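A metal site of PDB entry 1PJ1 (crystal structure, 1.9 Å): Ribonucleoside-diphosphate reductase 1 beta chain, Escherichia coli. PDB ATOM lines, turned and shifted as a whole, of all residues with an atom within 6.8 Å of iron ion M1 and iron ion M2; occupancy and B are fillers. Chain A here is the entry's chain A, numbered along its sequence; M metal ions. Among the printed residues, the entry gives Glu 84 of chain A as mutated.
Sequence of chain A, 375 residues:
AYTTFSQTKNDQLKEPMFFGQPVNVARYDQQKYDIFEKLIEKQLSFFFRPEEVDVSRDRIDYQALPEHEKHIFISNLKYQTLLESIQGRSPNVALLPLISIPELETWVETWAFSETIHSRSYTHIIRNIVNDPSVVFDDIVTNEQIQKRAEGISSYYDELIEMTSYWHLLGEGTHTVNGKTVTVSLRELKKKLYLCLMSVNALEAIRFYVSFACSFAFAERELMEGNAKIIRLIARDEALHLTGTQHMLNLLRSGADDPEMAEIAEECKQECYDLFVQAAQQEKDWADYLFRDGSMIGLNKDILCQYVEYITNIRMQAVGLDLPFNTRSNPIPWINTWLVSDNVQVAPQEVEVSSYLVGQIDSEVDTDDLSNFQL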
ATOM      1  N   GLN A  80      -6.573  27.105 -34.539  1.00  0.00           N
ATOM      2  CA  GLN A  80      -7.574  26.679 -33.561  1.00  0.00           C
ATOM      3  C   GLN A  80      -7.272  25.243 -33.140  1.00  0.00           C
ATOM      4  O   GLN A  80      -7.331  24.902 -31.956  1.00  0.00           O
ATOM      5  CB  GLN A  80      -8.989  26.765 -34.155  1.00  0.00           C
ATOM      6  CG  GLN A  80      -9.411  28.173 -34.612  1.00  0.00           C
ATOM      7  CD  GLN A  80     -10.784  28.215 -35.285  1.00  0.00           C
ATOM      8  OE1 GLN A  80     -11.096  27.391 -36.148  1.00  0.00           O
ATOM      9  NE2 GLN A  80     -11.613  29.178 -34.898  1.00  0.00           N
ATOM     10  N   LEU A  83      -4.334  25.158 -30.722  1.00  0.00           N
ATOM     11  CA  LEU A  83      -4.724  25.551 -29.367  1.00  0.00           C
ATOM     12  C   LEU A  83      -5.541  24.484 -28.639  1.00  0.00           C
ATOM     13  O   LEU A  83      -5.363  24.290 -27.426  1.00  0.00           O
ATOM     14  CB  LEU A  83      -5.502  26.868 -29.382  1.00  0.00           C
ATOM     15  CG  LEU A  83      -4.762  28.124 -29.864  1.00  0.00           C
ATOM     16  CD1 LEU A  83      -5.692  29.321 -29.731  1.00  0.00           C
ATOM     17  CD2 LEU A  83      -3.503  28.342 -29.029  1.00  0.00           C
ATOM     18  N   GLU A  84      -6.424  23.793 -29.352  1.00  0.00           N
ATOM     19  CA  GLU A  84      -7.238  22.750 -28.712  1.00  0.00           C
ATOM     20  C   GLU A  84      -6.369  21.551 -28.334  1.00  0.00           C
ATOM     21  O   GLU A  84      -6.592  20.927 -27.294  1.00  0.00           O
ATOM     22  CB  GLU A  84      -8.384  22.307 -29.647  1.00  0.00           C
ATOM     23  CG  GLU A  84      -9.360  23.420 -30.004  1.00  0.00           C
ATOM     24  CD  GLU A  84     -10.158  23.939 -28.823  1.00  0.00           C
ATOM     25  OE1 GLU A  84      -9.874  23.552 -27.667  1.00  0.00           O
ATOM     26  OE2 GLU A  84     -11.088  24.744 -29.059  1.00  0.00           O
ATOM     27  N   GLN A  87      -4.735  22.684 -25.204  1.00  0.00           N
ATOM     28  CA  GLN A  87      -5.677  22.829 -24.091  1.00  0.00           C
ATOM     29  C   GLN A  87      -6.349  21.529 -23.653  1.00  0.00           C
ATOM     30  O   GLN A  87      -6.885  21.446 -22.548  1.00  0.00           O
ATOM     31  CB  GLN A  87      -6.741  23.878 -24.441  1.00  0.00           C
ATOM     32  CG  GLN A  87      -6.196  25.315 -24.397  1.00  0.00           C
ATOM     33  CD  GLN A  87      -5.462  25.618 -23.096  1.00  0.00           C
ATOM     34  OE1 GLN A  87      -4.279  25.297 -22.954  1.00  0.00           O
ATOM     35  NE2 GLN A  87      -6.164  26.207 -22.140  1.00  0.00           N
ATOM     36  N   TRP A 111     -13.073  20.768 -17.911  1.00  0.00           N
ATOM     37  CA  TRP A 111     -12.685  21.825 -18.824  1.00  0.00           C
ATOM     38  C   TRP A 111     -11.786  21.212 -19.910  1.00  0.00           C
ATOM     39  O   TRP A 111     -12.058  21.323 -21.112  1.00  0.00           O
ATOM     40  CB  TRP A 111     -11.987  22.922 -18.000  1.00  0.00           C
ATOM     41  CG  TRP A 111     -11.084  23.876 -18.703  1.00  0.00           C
ATOM     42  CD1 TRP A 111     -11.068  24.202 -20.032  1.00  0.00           C
ATOM     43  CD2 TRP A 111     -10.084  24.679 -18.077  1.00  0.00           C
ATOM     44  NE1 TRP A 111     -10.116  25.169 -20.268  1.00  0.00           N
ATOM     45  CE2 TRP A 111      -9.498  25.480 -19.084  1.00  0.00           C
ATOM     46  CE3 TRP A 111      -9.624  24.816 -16.752  1.00  0.00           C
ATOM     47  CZ2 TRP A 111      -8.472  26.395 -18.814  1.00  0.00           C
ATOM     48  CZ3 TRP A 111      -8.598  25.731 -16.482  1.00  0.00           C
ATOM     49  CH2 TRP A 111      -8.039  26.506 -17.506  1.00  0.00           C
ATOM     50  N   SER A 114     -13.606  18.921 -22.362  1.00  0.00           N
ATOM     51  CA  SER A 114     -14.383  19.638 -23.378  1.00  0.00           C
ATOM     52  C   SER A 114     -13.468  20.107 -24.510  1.00  0.00           C
ATOM     53  O   SER A 114     -13.884  20.161 -25.670  1.00  0.00           O
ATOM     54  CB  SER A 114     -15.139  20.820 -22.748  1.00  0.00           C
ATOM     55  OG  SER A 114     -14.289  21.892 -22.400  1.00  0.00           O
ATOM     56  N   GLU A 115     -12.221  20.429 -24.187  1.00  0.00           N
ATOM     57  CA  GLU A 115     -11.278  20.877 -25.217  1.00  0.00           C
ATOM     58  C   GLU A 115     -10.960  19.713 -26.174  1.00  0.00           C
ATOM     59  O   GLU A 115     -10.748  19.928 -27.374  1.00  0.00           O
ATOM     60  CB  GLU A 115      -9.991  21.423 -24.584  1.00  0.00           C
ATOM     61  CG  GLU A 115     -10.224  22.494 -23.503  1.00  0.00           C
ATOM     62  CD  GLU A 115     -10.634  23.857 -24.052  1.00  0.00           C
ATOM     63  OE1 GLU A 115     -11.429  23.908 -25.011  1.00  0.00           O
ATOM     64  OE2 GLU A 115     -10.165  24.882 -23.512  1.00  0.00           O
ATOM     65  N   THR A 116     -10.938  18.473 -25.673  1.00  0.00           N
ATOM     66  CA  THR A 116     -10.666  17.342 -26.549  1.00  0.00           C
ATOM     67  C   THR A 116     -11.844  17.147 -27.495  1.00  0.00           C
ATOM     68  O   THR A 116     -11.677  16.687 -28.628  1.00  0.00           O
ATOM     69  CB  THR A 116     -10.398  16.024 -25.777  1.00  0.00           C
ATOM     70  OG1 THR A 116     -11.589  15.606 -25.099  1.00  0.00           O
ATOM     71  CG2 THR A 116      -9.270  16.228 -24.775  1.00  0.00           C
ATOM     72  N   HIS A 118     -13.501  19.589 -28.626  1.00  0.00           N
ATOM     73  CA  HIS A 118     -13.275  20.636 -29.614  1.00  0.00           C
ATOM     74  C   HIS A 118     -12.251  20.141 -30.644  1.00  0.00           C
ATOM     75  O   HIS A 118     -12.389  20.400 -31.838  1.00  0.00           O
ATOM     76  CB  HIS A 118     -12.777  21.901 -28.913  1.00  0.00           C
ATOM     77  CG  HIS A 118     -13.749  22.466 -27.926  1.00  0.00           C
ATOM     78  ND1 HIS A 118     -13.461  23.537 -27.125  1.00  0.00           N
ATOM     79  CD2 HIS A 118     -15.006  22.076 -27.602  1.00  0.00           C
ATOM     80  CE1 HIS A 118     -14.501  23.792 -26.338  1.00  0.00           C
ATOM     81  NE2 HIS A 118     -15.447  22.923 -26.611  1.00  0.00           N
ATOM     82  N   SER A 119     -11.238  19.417 -30.182  1.00  0.00           N
ATOM     83  CA  SER A 119     -10.240  18.866 -31.108  1.00  0.00           C
ATOM     84  C   SER A 119     -10.900  17.880 -32.059  1.00  0.00           C
ATOM     85  O   SER A 119     -10.622  17.875 -33.261  1.00  0.00           O
ATOM     86  CB  SER A 119      -9.118  18.154 -30.339  1.00  0.00           C
ATOM     87  OG  SER A 119      -8.315  19.076 -29.647  1.00  0.00           O
ATOM     88  N   TYR A 122     -12.733  19.626 -34.816  1.00  0.00           N
ATOM     89  CA  TYR A 122     -11.892  20.086 -35.911  1.00  0.00           C
ATOM     90  C   TYR A 122     -11.444  18.964 -36.854  1.00  0.00           C
ATOM     91  O   TYR A 122     -11.271  19.194 -38.052  1.00  0.00           O
ATOM     92  CB  TYR A 122     -10.694  20.865 -35.363  1.00  0.00           C
ATOM     93  CG  TYR A 122     -11.096  22.221 -34.834  1.00  0.00           C
ATOM     94  CD1 TYR A 122     -11.754  23.140 -35.660  1.00  0.00           C
ATOM     95  CD2 TYR A 122     -10.845  22.600 -33.506  1.00  0.00           C
ATOM     96  CE1 TYR A 122     -12.149  24.397 -35.179  1.00  0.00           C
ATOM     97  CE2 TYR A 122     -11.243  23.847 -33.022  1.00  0.00           C
ATOM     98  CZ  TYR A 122     -11.896  24.740 -33.863  1.00  0.00           C
ATOM     99  OH  TYR A 122     -12.292  25.980 -33.408  1.00  0.00           O
ATOM    100  N   GLU A 204      -7.681  31.577 -23.569  1.00  0.00           N
ATOM    101  CA  GLU A 204      -9.102  31.271 -23.602  1.00  0.00           C
ATOM    102  C   GLU A 204      -9.980  32.471 -23.992  1.00  0.00           C
ATOM    103  O   GLU A 204     -10.905  32.342 -24.795  1.00  0.00           O
ATOM    104  CB  GLU A 204      -9.578  30.779 -22.216  1.00  0.00           C
ATOM    105  CG  GLU A 204      -8.910  29.514 -21.676  1.00  0.00           C
ATOM    106  CD  GLU A 204      -9.462  28.234 -22.286  1.00  0.00           C
ATOM    107  OE1 GLU A 204     -10.534  28.273 -22.907  1.00  0.00           O
ATOM    108  OE2 GLU A 204      -8.805  27.176 -22.129  1.00  0.00           O
ATOM    109  N   PHE A 208      -8.769  32.491 -28.686  1.00  0.00           N
ATOM    110  CA  PHE A 208      -9.887  31.742 -29.264  1.00  0.00           C
ATOM    111  C   PHE A 208     -10.910  32.677 -29.934  1.00  0.00           C
ATOM    112  O   PHE A 208     -11.394  32.400 -31.030  1.00  0.00           O
ATOM    113  CB  PHE A 208     -10.624  30.898 -28.210  1.00  0.00           C
ATOM    114  CG  PHE A 208      -9.987  29.557 -27.934  1.00  0.00           C
ATOM    115  CD1 PHE A 208      -9.594  28.726 -28.985  1.00  0.00           C
ATOM    116  CD2 PHE A 208      -9.804  29.109 -26.628  1.00  0.00           C
ATOM    117  CE1 PHE A 208      -9.033  27.462 -28.735  1.00  0.00           C
ATOM    118  CE2 PHE A 208      -9.253  27.851 -26.370  1.00  0.00           C
ATOM    119  CZ  PHE A 208      -8.866  27.032 -27.425  1.00  0.00           C
ATOM    120  N   PHE A 212     -12.606  33.027 -33.722  1.00  0.00           N
ATOM    121  CA  PHE A 212     -14.034  32.874 -33.969  1.00  0.00           C
ATOM    122  C   PHE A 212     -14.524  33.912 -34.973  1.00  0.00           C
ATOM    123  O   PHE A 212     -15.359  33.608 -35.829  1.00  0.00           O
ATOM    124  CB  PHE A 212     -14.842  33.008 -32.674  1.00  0.00           C
ATOM    125  CG  PHE A 212     -14.580  31.925 -31.671  1.00  0.00           C
ATOM    126  CD1 PHE A 212     -14.094  30.693 -32.078  1.00  0.00           C
ATOM    127  CD2 PHE A 212     -14.840  32.128 -30.319  1.00  0.00           C
ATOM    128  CE1 PHE A 212     -13.863  29.672 -31.144  1.00  0.00           C
ATOM    129  CE2 PHE A 212     -14.622  31.132 -29.393  1.00  0.00           C
ATOM    130  CZ  PHE A 212     -14.126  29.897 -29.798  1.00  0.00           C
ATOM    131  N   ILE A 234     -18.487  25.509 -29.722  1.00  0.00           N
ATOM    132  CA  ILE A 234     -17.179  25.666 -29.094  1.00  0.00           C
ATOM    133  C   ILE A 234     -17.134  26.966 -28.301  1.00  0.00           C
ATOM    134  O   ILE A 234     -16.744  26.966 -27.136  1.00  0.00           O
ATOM    135  CB  ILE A 234     -16.061  25.631 -30.145  1.00  0.00           C
ATOM    136  CG1 ILE A 234     -16.013  24.242 -30.784  1.00  0.00           C
ATOM    137  CG2 ILE A 234     -14.709  25.992 -29.501  1.00  0.00           C
ATOM    138  CD1 ILE A 234     -14.957  24.104 -31.866  1.00  0.00           C
ATOM    139  N   ASP A 237     -18.573  26.877 -24.967  1.00  0.00           N
ATOM    140  CA  ASP A 237     -17.711  26.259 -23.946  1.00  0.00           C
ATOM    141  C   ASP A 237     -16.603  27.223 -23.504  1.00  0.00           C
ATOM    142  O   ASP A 237     -16.333  27.360 -22.311  1.00  0.00           O
ATOM    143  CB  ASP A 237     -17.069  24.977 -24.480  1.00  0.00           C
ATOM    144  CG  ASP A 237     -18.084  23.860 -24.710  1.00  0.00           C
ATOM    145  OD1 ASP A 237     -19.184  23.920 -24.129  1.00  0.00           O
ATOM    146  OD2 ASP A 237     -17.759  22.904 -25.437  1.00  0.00           O
ATOM    147  N   GLU A 238     -15.962  27.895 -24.463  1.00  0.00           N
ATOM    148  CA  GLU A 238     -14.882  28.814 -24.127  1.00  0.00           C
ATOM    149  C   GLU A 238     -15.347  29.907 -23.147  1.00  0.00           C
ATOM    150  O   GLU A 238     -14.565  30.387 -22.319  1.00  0.00           O
ATOM    151  CB  GLU A 238     -14.291  29.464 -25.386  1.00  0.00           C
ATOM    152  CG  GLU A 238     -13.758  28.503 -26.443  1.00  0.00           C
ATOM    153  CD  GLU A 238     -12.780  27.460 -25.907  1.00  0.00           C
ATOM    154  OE1 GLU A 238     -12.227  27.658 -24.805  1.00  0.00           O
ATOM    155  OE2 GLU A 238     -12.579  26.438 -26.599  1.00  0.00           O
ATOM    156  N   ALA A 239     -16.618  30.301 -23.254  1.00  0.00           N
ATOM    157  CA  ALA A 239     -17.166  31.320 -22.357  1.00  0.00           C
ATOM    158  C   ALA A 239     -17.121  30.823 -20.907  1.00  0.00           C
ATOM    159  O   ALA A 239     -16.848  31.600 -19.974  1.00  0.00           O
ATOM    160  CB  ALA A 239     -18.588  31.655 -22.753  1.00  0.00           C
ATOM    161  N   HIS A 241     -15.019  28.447 -19.811  1.00  0.00           N
ATOM    162  CA  HIS A 241     -13.608  28.312 -19.464  1.00  0.00           C
ATOM    163  C   HIS A 241     -13.007  29.633 -18.994  1.00  0.00           C
ATOM    164  O   HIS A 241     -12.319  29.677 -17.976  1.00  0.00           O
ATOM    165  CB  HIS A 241     -12.812  27.779 -20.663  1.00  0.00           C
ATOM    166  CG  HIS A 241     -13.325  26.472 -21.179  1.00  0.00           C
ATOM    167  ND1 HIS A 241     -12.898  25.925 -22.369  1.00  0.00           N
ATOM    168  CD2 HIS A 241     -14.240  25.601 -20.674  1.00  0.00           C
ATOM    169  CE1 HIS A 241     -13.527  24.787 -22.587  1.00  0.00           C
ATOM    170  NE2 HIS A 241     -14.340  24.559 -21.577  1.00  0.00           N
ATOM    171  N   LEU A 242     -13.268  30.709 -19.716  1.00  0.00           N
ATOM    172  CA  LEU A 242     -12.710  31.986 -19.322  1.00  0.00           C
ATOM    173  C   LEU A 242     -13.396  32.505 -18.048  1.00  0.00           C
ATOM    174  O   LEU A 242     -12.789  33.217 -17.252  1.00  0.00           O
ATOM    175  CB  LEU A 242     -12.799  32.997 -20.467  1.00  0.00           C
ATOM    176  CG  LEU A 242     -14.113  33.650 -20.869  1.00  0.00           C
ATOM    177  CD1 LEU A 242     -14.438  34.796 -19.908  1.00  0.00           C
ATOM    178  CD2 LEU A 242     -13.992  34.177 -22.299  1.00  0.00           C
HETATM  179 FE    FE M   1     -11.287  26.512 -23.471  1.00  0.00          FE
HETATM  180 FE    FE M   2     -11.693  24.666 -26.959  1.00  0.00          FE
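OE2 of Glu 115 is bound to iron ion M1, 2.0 Å away. OE1 of Glu 238 binds iron ion M1, 2.0 Å away. OE1 of Glu 204 is bound to iron ion M1 (2.0 Å). ND1 of His 241 is bound to iron ion M1 (2.0 Å). Iron ion M1 has four donor atoms within binding distance.
Iron ion M2 is bound by OE2 of Glu 238, ND1 of His 118, OE1 of Glu 115, OE2 of Glu 84 and OE1 of Glu 84. Iron ion M2 has five donor atoms within binding distance.
O of Glu 84 sits close to OG of Ser 119 (3.5 Å). A ring nitrogen (NE2) of His 241 sits at hydrogen-bond distance from the side-chain hydroxyl (OG) of Ser 114, at 2.8 Å. The side-chain carboxylate of Glu 204 is in hydrogen-bond range of the side-chain amide nitrogen of Gln 87 (2.8 Å). O of Trp 111 is in hydrogen-bond range of OG of Ser 114, 2.6 Å away. OE2 of Glu 204 sits at hydrogen-bond distance from NE1 of Trp 111. NE2 of His 118 sits close to O of Ser 114 (3.3 Å). The side-chain hydroxyl (OG) of Ser 119 sits at hydrogen-bond distance from the backbone carbonyl oxygen (O) of Glu 115 (3.4 Å). OD2 of Asp 237 lies within hydrogen-bond range of NE2 of His 118 (2.6 Å).
CZ of Phe 208 touches iron ion M2 (3.7 Å). Five residues have an atom within 4 Å of iron ion M2: Glu 84, Glu 115, His 118, Phe 208 and Glu 238. The nearest printed residue that does not touch iron ion M2 is Ile 234 (4.2 Å).
Residues that only touch iron ion M1: Trp 111 (3.7 Å) and Phe 208 (3.8 Å).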
